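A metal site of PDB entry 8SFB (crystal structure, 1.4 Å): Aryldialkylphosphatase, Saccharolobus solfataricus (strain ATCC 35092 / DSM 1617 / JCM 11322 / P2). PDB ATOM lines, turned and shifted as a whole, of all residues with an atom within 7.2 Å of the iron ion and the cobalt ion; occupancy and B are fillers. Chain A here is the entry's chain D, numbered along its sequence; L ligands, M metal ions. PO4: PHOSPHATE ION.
OG1 of Thr 68 sits at hydrogen-bond distance from ND1 of His 24, 2.7 Å away.
The backbone NH (N) of His 24 lies within hydrogen-bond range of the backbone carbonyl oxygen (O) of Tyr 257 (2.9 Å).
NE2 of His 170 lies within hydrogen-bond range of OD1 of Asp 141, 2.8 Å away.
The backbone carbonyl oxygen (O) of Ile 138 sits at hydrogen-bond distance from the backbone NH (N) of His 170, 2.8 Å away.
A ring nitrogen (ND1) of His 199 lies within hydrogen-bond range of the guanidinium group (NE) of Arg 223 (3.4 Å).
OD1 of Asp 222 sits at hydrogen-bond distance from ND1 of His 199 (2.7 Å).
NE of Arg 223 is in salt-bridge range of OD2 of Asp 256.
N of Asp 256 lies within hydrogen-bond range of OE2 of Glu 23 (3.3 Å).
Within 4 Å of the iron ion: His 22, His 24, KCX 137 and Asp 256.
The nearest printed residue that does not touch the iron ion is His 199 (4.3 Å).
Arg 223 touches the cobalt ion.
Within 4 Å of the cobalt ion: KCX 137, His 170, His 199 and Arg 223.
The iron ion is bound by an oxygen (O2) of the ligand, an oxygen (O3) of the ligand, a ring nitrogen (NE2) of His 24, OQ1 of KCX 137, a ring nitrogen (NE2) of His 22 and the side-chain carboxylate of Asp 256.
The cobalt ion is bound by O4 of the ligand, O2 of the ligand, ND1 of His 170, OQ2 of KCX 137 and NE2 of His 199.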
ATOM      1  N   HIS A  22      21.865   4.652  21.039  1.00  0.00           N
ATOM      2  CA  HIS A  22      20.873   3.877  21.786  1.00  0.00           C
ATOM      3  C   HIS A  22      19.488   4.460  21.526  1.00  0.00           C
ATOM      4  O   HIS A  22      19.019   5.323  22.260  1.00  0.00           O
ATOM      5  CB  HIS A  22      21.219   3.867  23.279  1.00  0.00           C
ATOM      6  CG  HIS A  22      20.403   2.904  24.085  1.00  0.00           C
ATOM      7  ND1 HIS A  22      20.943   2.135  25.095  1.00  0.00           N
ATOM      8  CD2 HIS A  22      19.087   2.587  24.042  1.00  0.00           C
ATOM      9  CE1 HIS A  22      19.992   1.388  25.634  1.00  0.00           C
ATOM     10  NE2 HIS A  22      18.862   1.650  25.018  1.00  0.00           N
ATOM     11  N   GLU A  23      18.841   3.944  20.468  1.00  0.00           N
ATOM     12  CA  GLU A  23      17.478   4.311  20.111  1.00  0.00           C
ATOM     13  C   GLU A  23      16.727   3.051  19.719  1.00  0.00           C
ATOM     14  O   GLU A  23      17.345   2.055  19.337  1.00  0.00           O
ATOM     15  CB  GLU A  23      17.430   5.308  18.944  1.00  0.00           C
ATOM     16  CG  GLU A  23      18.343   6.516  19.123  1.00  0.00           C
ATOM     17  CD  GLU A  23      17.945   7.452  20.258  1.00  0.00           C
ATOM     18  OE1 GLU A  23      18.764   8.309  20.624  1.00  0.00           O
ATOM     19  OE2 GLU A  23      16.796   7.343  20.741  1.00  0.00           O
ATOM     20  N   HIS A  24      15.396   3.091  19.795  1.00  0.00           N
ATOM     21  CA  HIS A  24      14.567   1.945  19.457  1.00  0.00           C
ATOM     22  C   HIS A  24      13.546   2.342  18.403  1.00  0.00           C
ATOM     23  O   HIS A  24      12.733   3.240  18.633  1.00  0.00           O
ATOM     24  CB  HIS A  24      13.840   1.426  20.702  1.00  0.00           C
ATOM     25  CG  HIS A  24      14.755   0.950  21.787  1.00  0.00           C
ATOM     26  ND1 HIS A  24      15.312  -0.314  21.797  1.00  0.00           N
ATOM     27  CD2 HIS A  24      15.163   1.551  22.912  1.00  0.00           C
ATOM     28  CE1 HIS A  24      16.051  -0.447  22.898  1.00  0.00           C
ATOM     29  NE2 HIS A  24      15.987   0.683  23.587  1.00  0.00           N
ATOM     30  N   PRO A  67      19.376  -1.067  20.096  1.00  0.00           N
ATOM     31  CA  PRO A  67      19.608  -2.233  20.937  1.00  0.00           C
ATOM     32  C   PRO A  67      18.337  -2.944  21.390  1.00  0.00           C
ATOM     33  O   PRO A  67      18.246  -3.391  22.532  1.00  0.00           O
ATOM     34  CB  PRO A  67      20.373  -1.641  22.127  1.00  0.00           C
ATOM     35  CG  PRO A  67      19.773  -0.268  22.267  1.00  0.00           C
ATOM     36  CD  PRO A  67      19.447   0.187  20.858  1.00  0.00           C
ATOM     37  N   THR A  68      17.352  -3.060  20.478  1.00  0.00           N
ATOM     38  CA  THR A  68      16.175  -3.871  20.737  1.00  0.00           C
ATOM     39  C   THR A  68      16.575  -5.336  20.550  1.00  0.00           C
ATOM     40  O   THR A  68      17.039  -5.698  19.471  1.00  0.00           O
ATOM     41  CB  THR A  68      15.025  -3.498  19.789  1.00  0.00           C
ATOM     42  OG1 THR A  68      14.763  -2.092  19.832  1.00  0.00           O
ATOM     43  CG2 THR A  68      13.754  -4.235  20.120  1.00  0.00           C
ATOM     44  N   CYS A  72      12.301  -7.361  24.158  1.00  0.00           N
ATOM     45  CA  CYS A  72      11.770  -6.081  23.717  1.00  0.00           C
ATOM     46  C   CYS A  72      11.346  -6.120  22.246  1.00  0.00           C
ATOM     47  O   CYS A  72      11.074  -5.069  21.659  1.00  0.00           O
ATOM     48  CB  CYS A  72      12.782  -4.970  23.969  1.00  0.00           C
ATOM     49  SG  CYS A  72      12.972  -4.594  25.719  1.00  0.00           S
ATOM     50  N   ILE A  97      17.286  -9.137  27.247  1.00  0.00           N
ATOM     51  CA  ILE A  97      16.909  -8.263  28.349  1.00  0.00           C
ATOM     52  C   ILE A  97      16.059  -9.056  29.330  1.00  0.00           C
ATOM     53  O   ILE A  97      14.907  -9.378  29.040  1.00  0.00           O
ATOM     54  CB  ILE A  97      16.128  -7.024  27.860  1.00  0.00           C
ATOM     55  CG1 ILE A  97      16.876  -6.267  26.763  1.00  0.00           C
ATOM     56  CG2 ILE A  97      15.759  -6.117  29.031  1.00  0.00           C
ATOM     57  CD1 ILE A  97      18.197  -5.730  27.174  1.00  0.00           C
ATOM     58  N   PHE A  99      15.400  -9.086  33.837  1.00  0.00           N
ATOM     59  CA  PHE A  99      15.716  -8.495  35.130  1.00  0.00           C
ATOM     60  C   PHE A  99      15.801  -9.546  36.239  1.00  0.00           C
ATOM     61  O   PHE A  99      16.408  -9.282  37.280  1.00  0.00           O
ATOM     62  CB  PHE A  99      14.681  -7.437  35.531  1.00  0.00           C
ATOM     63  CG  PHE A  99      14.658  -6.213  34.655  1.00  0.00           C
ATOM     64  CD1 PHE A  99      15.637  -6.000  33.693  1.00  0.00           C
ATOM     65  CD2 PHE A  99      13.674  -5.259  34.811  1.00  0.00           C
ATOM     66  CE1 PHE A  99      15.609  -4.873  32.886  1.00  0.00           C
ATOM     67  CE2 PHE A  99      13.648  -4.121  34.013  1.00  0.00           C
ATOM     68  CZ  PHE A  99      14.614  -3.928  33.045  1.00  0.00           C
ATOM     69  N   KCX A 137      23.609  -6.845  23.561  1.00  0.00           N
ATOM     70  CA  KCX A 137      22.880  -6.054  24.581  1.00  0.00           C
ATOM     71  CB  KCX A 137      21.654  -5.423  23.928  1.00  0.00           C
ATOM     72  CG  KCX A 137      20.702  -4.725  24.885  1.00  0.00           C
ATOM     73  CD  KCX A 137      21.342  -3.531  25.537  1.00  0.00           C
ATOM     74  CE  KCX A 137      20.375  -2.786  26.433  1.00  0.00           C
ATOM     75  NZ  KCX A 137      19.192  -2.279  25.714  1.00  0.00           N
ATOM     76  C   KCX A 137      22.485  -6.960  25.742  1.00  0.00           C
ATOM     77  O   KCX A 137      21.922  -8.022  25.508  1.00  0.00           O
ATOM     78  CX  KCX A 137      18.358  -1.421  26.313  1.00  0.00           C
ATOM     79  OQ1 KCX A 137      17.330  -1.055  25.603  1.00  0.00           O
ATOM     80  OQ2 KCX A 137      18.540  -1.019  27.453  1.00  0.00           O
ATOM     81  N   ILE A 138      22.750  -6.483  26.961  1.00  0.00           N
ATOM     82  CA  ILE A 138      22.400  -7.225  28.205  1.00  0.00           C
ATOM     83  C   ILE A 138      21.827  -6.225  29.216  1.00  0.00           C
ATOM     84  O   ILE A 138      21.954  -5.025  29.016  1.00  0.00           O
ATOM     85  CB  ILE A 138      23.630  -7.939  28.800  1.00  0.00           C
ATOM     86  CG1 ILE A 138      24.710  -6.930  29.206  1.00  0.00           C
ATOM     87  CG2 ILE A 138      24.154  -8.995  27.846  1.00  0.00           C
ATOM     88  CD1 ILE A 138      25.931  -7.541  29.839  1.00  0.00           C
ATOM     89  N   ALA A 139      21.226  -6.733  30.304  1.00  0.00           N
ATOM     90  CA  ALA A 139      20.500  -5.897  31.249  1.00  0.00           C
ATOM     91  C   ALA A 139      20.656  -6.379  32.681  1.00  0.00           C
ATOM     92  O   ALA A 139      20.920  -7.547  32.956  1.00  0.00           O
ATOM     93  CB  ALA A 139      19.025  -5.838  30.916  1.00  0.00           C
ATOM     94  N   ASP A 141      18.572  -4.676  36.525  1.00  0.00           N
ATOM     95  CA  ASP A 141      17.815  -3.553  37.039  1.00  0.00           C
ATOM     96  C   ASP A 141      17.667  -3.679  38.550  1.00  0.00           C
ATOM     97  O   ASP A 141      18.608  -4.076  39.242  1.00  0.00           O
ATOM     98  CB  ASP A 141      16.470  -3.446  36.320  1.00  0.00           C
ATOM     99  CG  ASP A 141      15.914  -2.032  36.302  1.00  0.00           C
ATOM    100  OD1 ASP A 141      16.211  -1.285  35.339  1.00  0.00           O
ATOM    101  OD2 ASP A 141      15.202  -1.666  37.257  1.00  0.00           O
ATOM    102  N   THR A 169      24.882  -2.108  27.653  1.00  0.00           N
ATOM    103  CA  THR A 169      24.094  -2.584  28.776  1.00  0.00           C
ATOM    104  C   THR A 169      22.933  -1.650  29.092  1.00  0.00           C
ATOM    105  O   THR A 169      22.950  -0.455  28.786  1.00  0.00           O
ATOM    106  CB  THR A 169      24.935  -2.828  30.044  1.00  0.00           C
ATOM    107  OG1 THR A 169      25.006  -1.625  30.808  1.00  0.00           O
ATOM    108  CG2 THR A 169      26.332  -3.333  29.728  1.00  0.00           C
ATOM    109  N   HIS A 170      21.920  -2.263  29.702  1.00  0.00           N
ATOM    110  CA  HIS A 170      20.884  -1.595  30.455  1.00  0.00           C
ATOM    111  C   HIS A 170      21.231  -1.776  31.926  1.00  0.00           C
ATOM    112  O   HIS A 170      21.467  -2.895  32.371  1.00  0.00           O
ATOM    113  CB  HIS A 170      19.556  -2.295  30.188  1.00  0.00           C
ATOM    114  CG  HIS A 170      18.444  -1.871  31.066  1.00  0.00           C
ATOM    115  ND1 HIS A 170      17.382  -1.121  30.603  1.00  0.00           N
ATOM    116  CD2 HIS A 170      18.214  -2.078  32.375  1.00  0.00           C
ATOM    117  CE1 HIS A 170      16.544  -0.902  31.598  1.00  0.00           C
ATOM    118  NE2 HIS A 170      17.026  -1.465  32.694  1.00  0.00           N
ATOM    119  N   SER A 171      21.284  -0.674  32.669  1.00  0.00           N
ATOM    120  CA  SER A 171      21.491  -0.766  34.109  1.00  0.00           C
ATOM    121  C   SER A 171      20.495   0.120  34.841  1.00  0.00           C
ATOM    122  O   SER A 171      19.787   0.920  34.223  1.00  0.00           O
ATOM    123  CB  SER A 171      22.932  -0.440  34.523  1.00  0.00           C
ATOM    124  OG  SER A 171      23.161   0.958  34.637  1.00  0.00           O
ATOM    125  N   GLY A 198      24.813   1.475  30.349  1.00  0.00           N
ATOM    126  CA  GLY A 198      23.657   2.283  29.999  1.00  0.00           C
ATOM    127  C   GLY A 198      22.908   2.863  31.200  1.00  0.00           C
ATOM    128  O   GLY A 198      22.964   2.344  32.319  1.00  0.00           O
ATOM    129  N   HIS A 199      22.214   3.962  30.904  1.00  0.00           N
ATOM    130  CA  HIS A 199      21.200   4.574  31.747  1.00  0.00           C
ATOM    131  C   HIS A 199      21.825   5.268  32.946  1.00  0.00           C
ATOM    132  O   HIS A 199      21.151   5.516  33.940  1.00  0.00           O
ATOM    133  CB  HIS A 199      20.129   3.559  32.155  1.00  0.00           C
ATOM    134  CG  HIS A 199      19.531   2.856  30.981  1.00  0.00           C
ATOM    135  ND1 HIS A 199      19.499   3.388  29.710  1.00  0.00           N
ATOM    136  CD2 HIS A 199      18.924   1.654  30.910  1.00  0.00           C
ATOM    137  CE1 HIS A 199      18.916   2.514  28.893  1.00  0.00           C
ATOM    138  NE2 HIS A 199      18.559   1.463  29.598  1.00  0.00           N
ATOM    139  N   ASP A 222      22.170   8.308  28.160  1.00  0.00           N
ATOM    140  CA  ASP A 222      21.146   8.088  27.181  1.00  0.00           C
ATOM    141  C   ASP A 222      19.930   8.872  27.664  1.00  0.00           C
ATOM    142  O   ASP A 222      19.902  10.149  27.581  1.00  0.00           O
ATOM    143  CB  ASP A 222      20.941   6.583  26.932  1.00  0.00           C
ATOM    144  CG  ASP A 222      21.214   5.718  28.159  1.00  0.00           C
ATOM    145  OD1 ASP A 222      20.470   5.855  29.125  1.00  0.00           O
ATOM    146  OD2 ASP A 222      22.173   4.901  28.136  1.00  0.00           O
ATOM    147  N   ARG A 223      19.004   8.140  28.299  1.00  0.00           N
ATOM    148  CA  ARG A 223      17.579   8.425  28.272  1.00  0.00           C
ATOM    149  C   ARG A 223      17.223   9.916  28.220  1.00  0.00           C
ATOM    150  O   ARG A 223      16.322  10.341  28.952  1.00  0.00           O
ATOM    151  CB  ARG A 223      16.939   7.732  29.463  1.00  0.00           C
ATOM    152  CG  ARG A 223      17.288   6.250  29.486  1.00  0.00           C
ATOM    153  CD  ARG A 223      16.781   5.539  30.716  1.00  0.00           C
ATOM    154  NE  ARG A 223      16.269   4.238  30.337  1.00  0.00           N
ATOM    155  CZ  ARG A 223      15.935   3.296  31.206  1.00  0.00           C
ATOM    156  NH1 ARG A 223      16.159   3.496  32.492  1.00  0.00           N
ATOM    157  NH2 ARG A 223      15.395   2.164  30.784  1.00  0.00           N
ATOM    158  N   ASP A 256      17.267   7.036  23.943  1.00  0.00           N
ATOM    159  CA  ASP A 256      16.617   5.776  24.279  1.00  0.00           C
ATOM    160  C   ASP A 256      15.159   5.901  23.887  1.00  0.00           C
ATOM    161  O   ASP A 256      14.284   5.309  24.512  1.00  0.00           O
ATOM    162  CB  ASP A 256      16.757   5.476  25.757  1.00  0.00           C
ATOM    163  CG  ASP A 256      16.562   4.027  26.153  1.00  0.00           C
ATOM    164  OD1 ASP A 256      16.362   3.197  25.257  1.00  0.00           O
ATOM    165  OD2 ASP A 256      16.600   3.742  27.347  1.00  0.00           O
ATOM    166  N   TYR A 257      14.913   6.707  22.852  1.00  0.00           N
ATOM    167  CA  TYR A 257      13.553   6.980  22.428  1.00  0.00           C
ATOM    168  C   TYR A 257      13.007   5.733  21.745  1.00  0.00           C
ATOM    169  O   TYR A 257      13.696   5.096  20.964  1.00  0.00           O
ATOM    170  CB  TYR A 257      13.500   8.180  21.478  1.00  0.00           C
ATOM    171  CG  TYR A 257      12.095   8.577  21.110  1.00  0.00           C
ATOM    172  CD1 TYR A 257      11.243   9.094  22.072  1.00  0.00           C
ATOM    173  CD2 TYR A 257      11.603   8.388  19.829  1.00  0.00           C
ATOM    174  CE1 TYR A 257       9.944   9.444  21.762  1.00  0.00           C
ATOM    175  CE2 TYR A 257      10.309   8.737  19.497  1.00  0.00           C
ATOM    176  CZ  TYR A 257       9.479   9.274  20.463  1.00  0.00           C
ATOM    177  OH  TYR A 257       8.190   9.624  20.151  1.00  0.00           O
ATOM    178  N   TRP A 263       4.362  -0.402  26.566  1.00  0.00           N
ATOM    179  CA  TRP A 263       4.223  -0.232  28.008  1.00  0.00           C
ATOM    180  C   TRP A 263       3.015   0.652  28.307  1.00  0.00           C
ATOM    181  O   TRP A 263       2.775   1.646  27.612  1.00  0.00           O
ATOM    182  CB  TRP A 263       5.491   0.377  28.615  1.00  0.00           C
ATOM    183  CG  TRP A 263       6.740  -0.432  28.394  1.00  0.00           C
ATOM    184  CD1 TRP A 263       6.833  -1.658  27.786  1.00  0.00           C
ATOM    185  CD2 TRP A 263       8.072  -0.076  28.781  1.00  0.00           C
ATOM    186  NE1 TRP A 263       8.133  -2.085  27.779  1.00  0.00           N
ATOM    187  CE2 TRP A 263       8.922  -1.134  28.385  1.00  0.00           C
ATOM    188  CE3 TRP A 263       8.639   1.029  29.435  1.00  0.00           C
ATOM    189  CZ2 TRP A 263      10.298  -1.118  28.604  1.00  0.00           C
ATOM    190  CZ3 TRP A 263      10.005   1.045  29.657  1.00  0.00           C
ATOM    191  CH2 TRP A 263      10.812  -0.013  29.252  1.00  0.00           C
HETATM  192  P   PO4 L   1      15.577   0.644  27.566  1.00  0.00           P
HETATM  193  O1  PO4 L   1      14.691   1.769  28.102  1.00  0.00           O
HETATM  194  O2  PO4 L   1      17.002   1.150  27.416  1.00  0.00           O
HETATM  195  O3  PO4 L   1      15.060   0.200  26.203  1.00  0.00           O
HETATM  196  O4  PO4 L   1      15.564  -0.535  28.542  1.00  0.00           O
HETATM  197 FE    FE M   1      16.808   1.013  25.468  1.00  0.00          FE
HETATM  198 CO    CO M   2      17.315  -0.036  28.826  1.00  0.00          CO
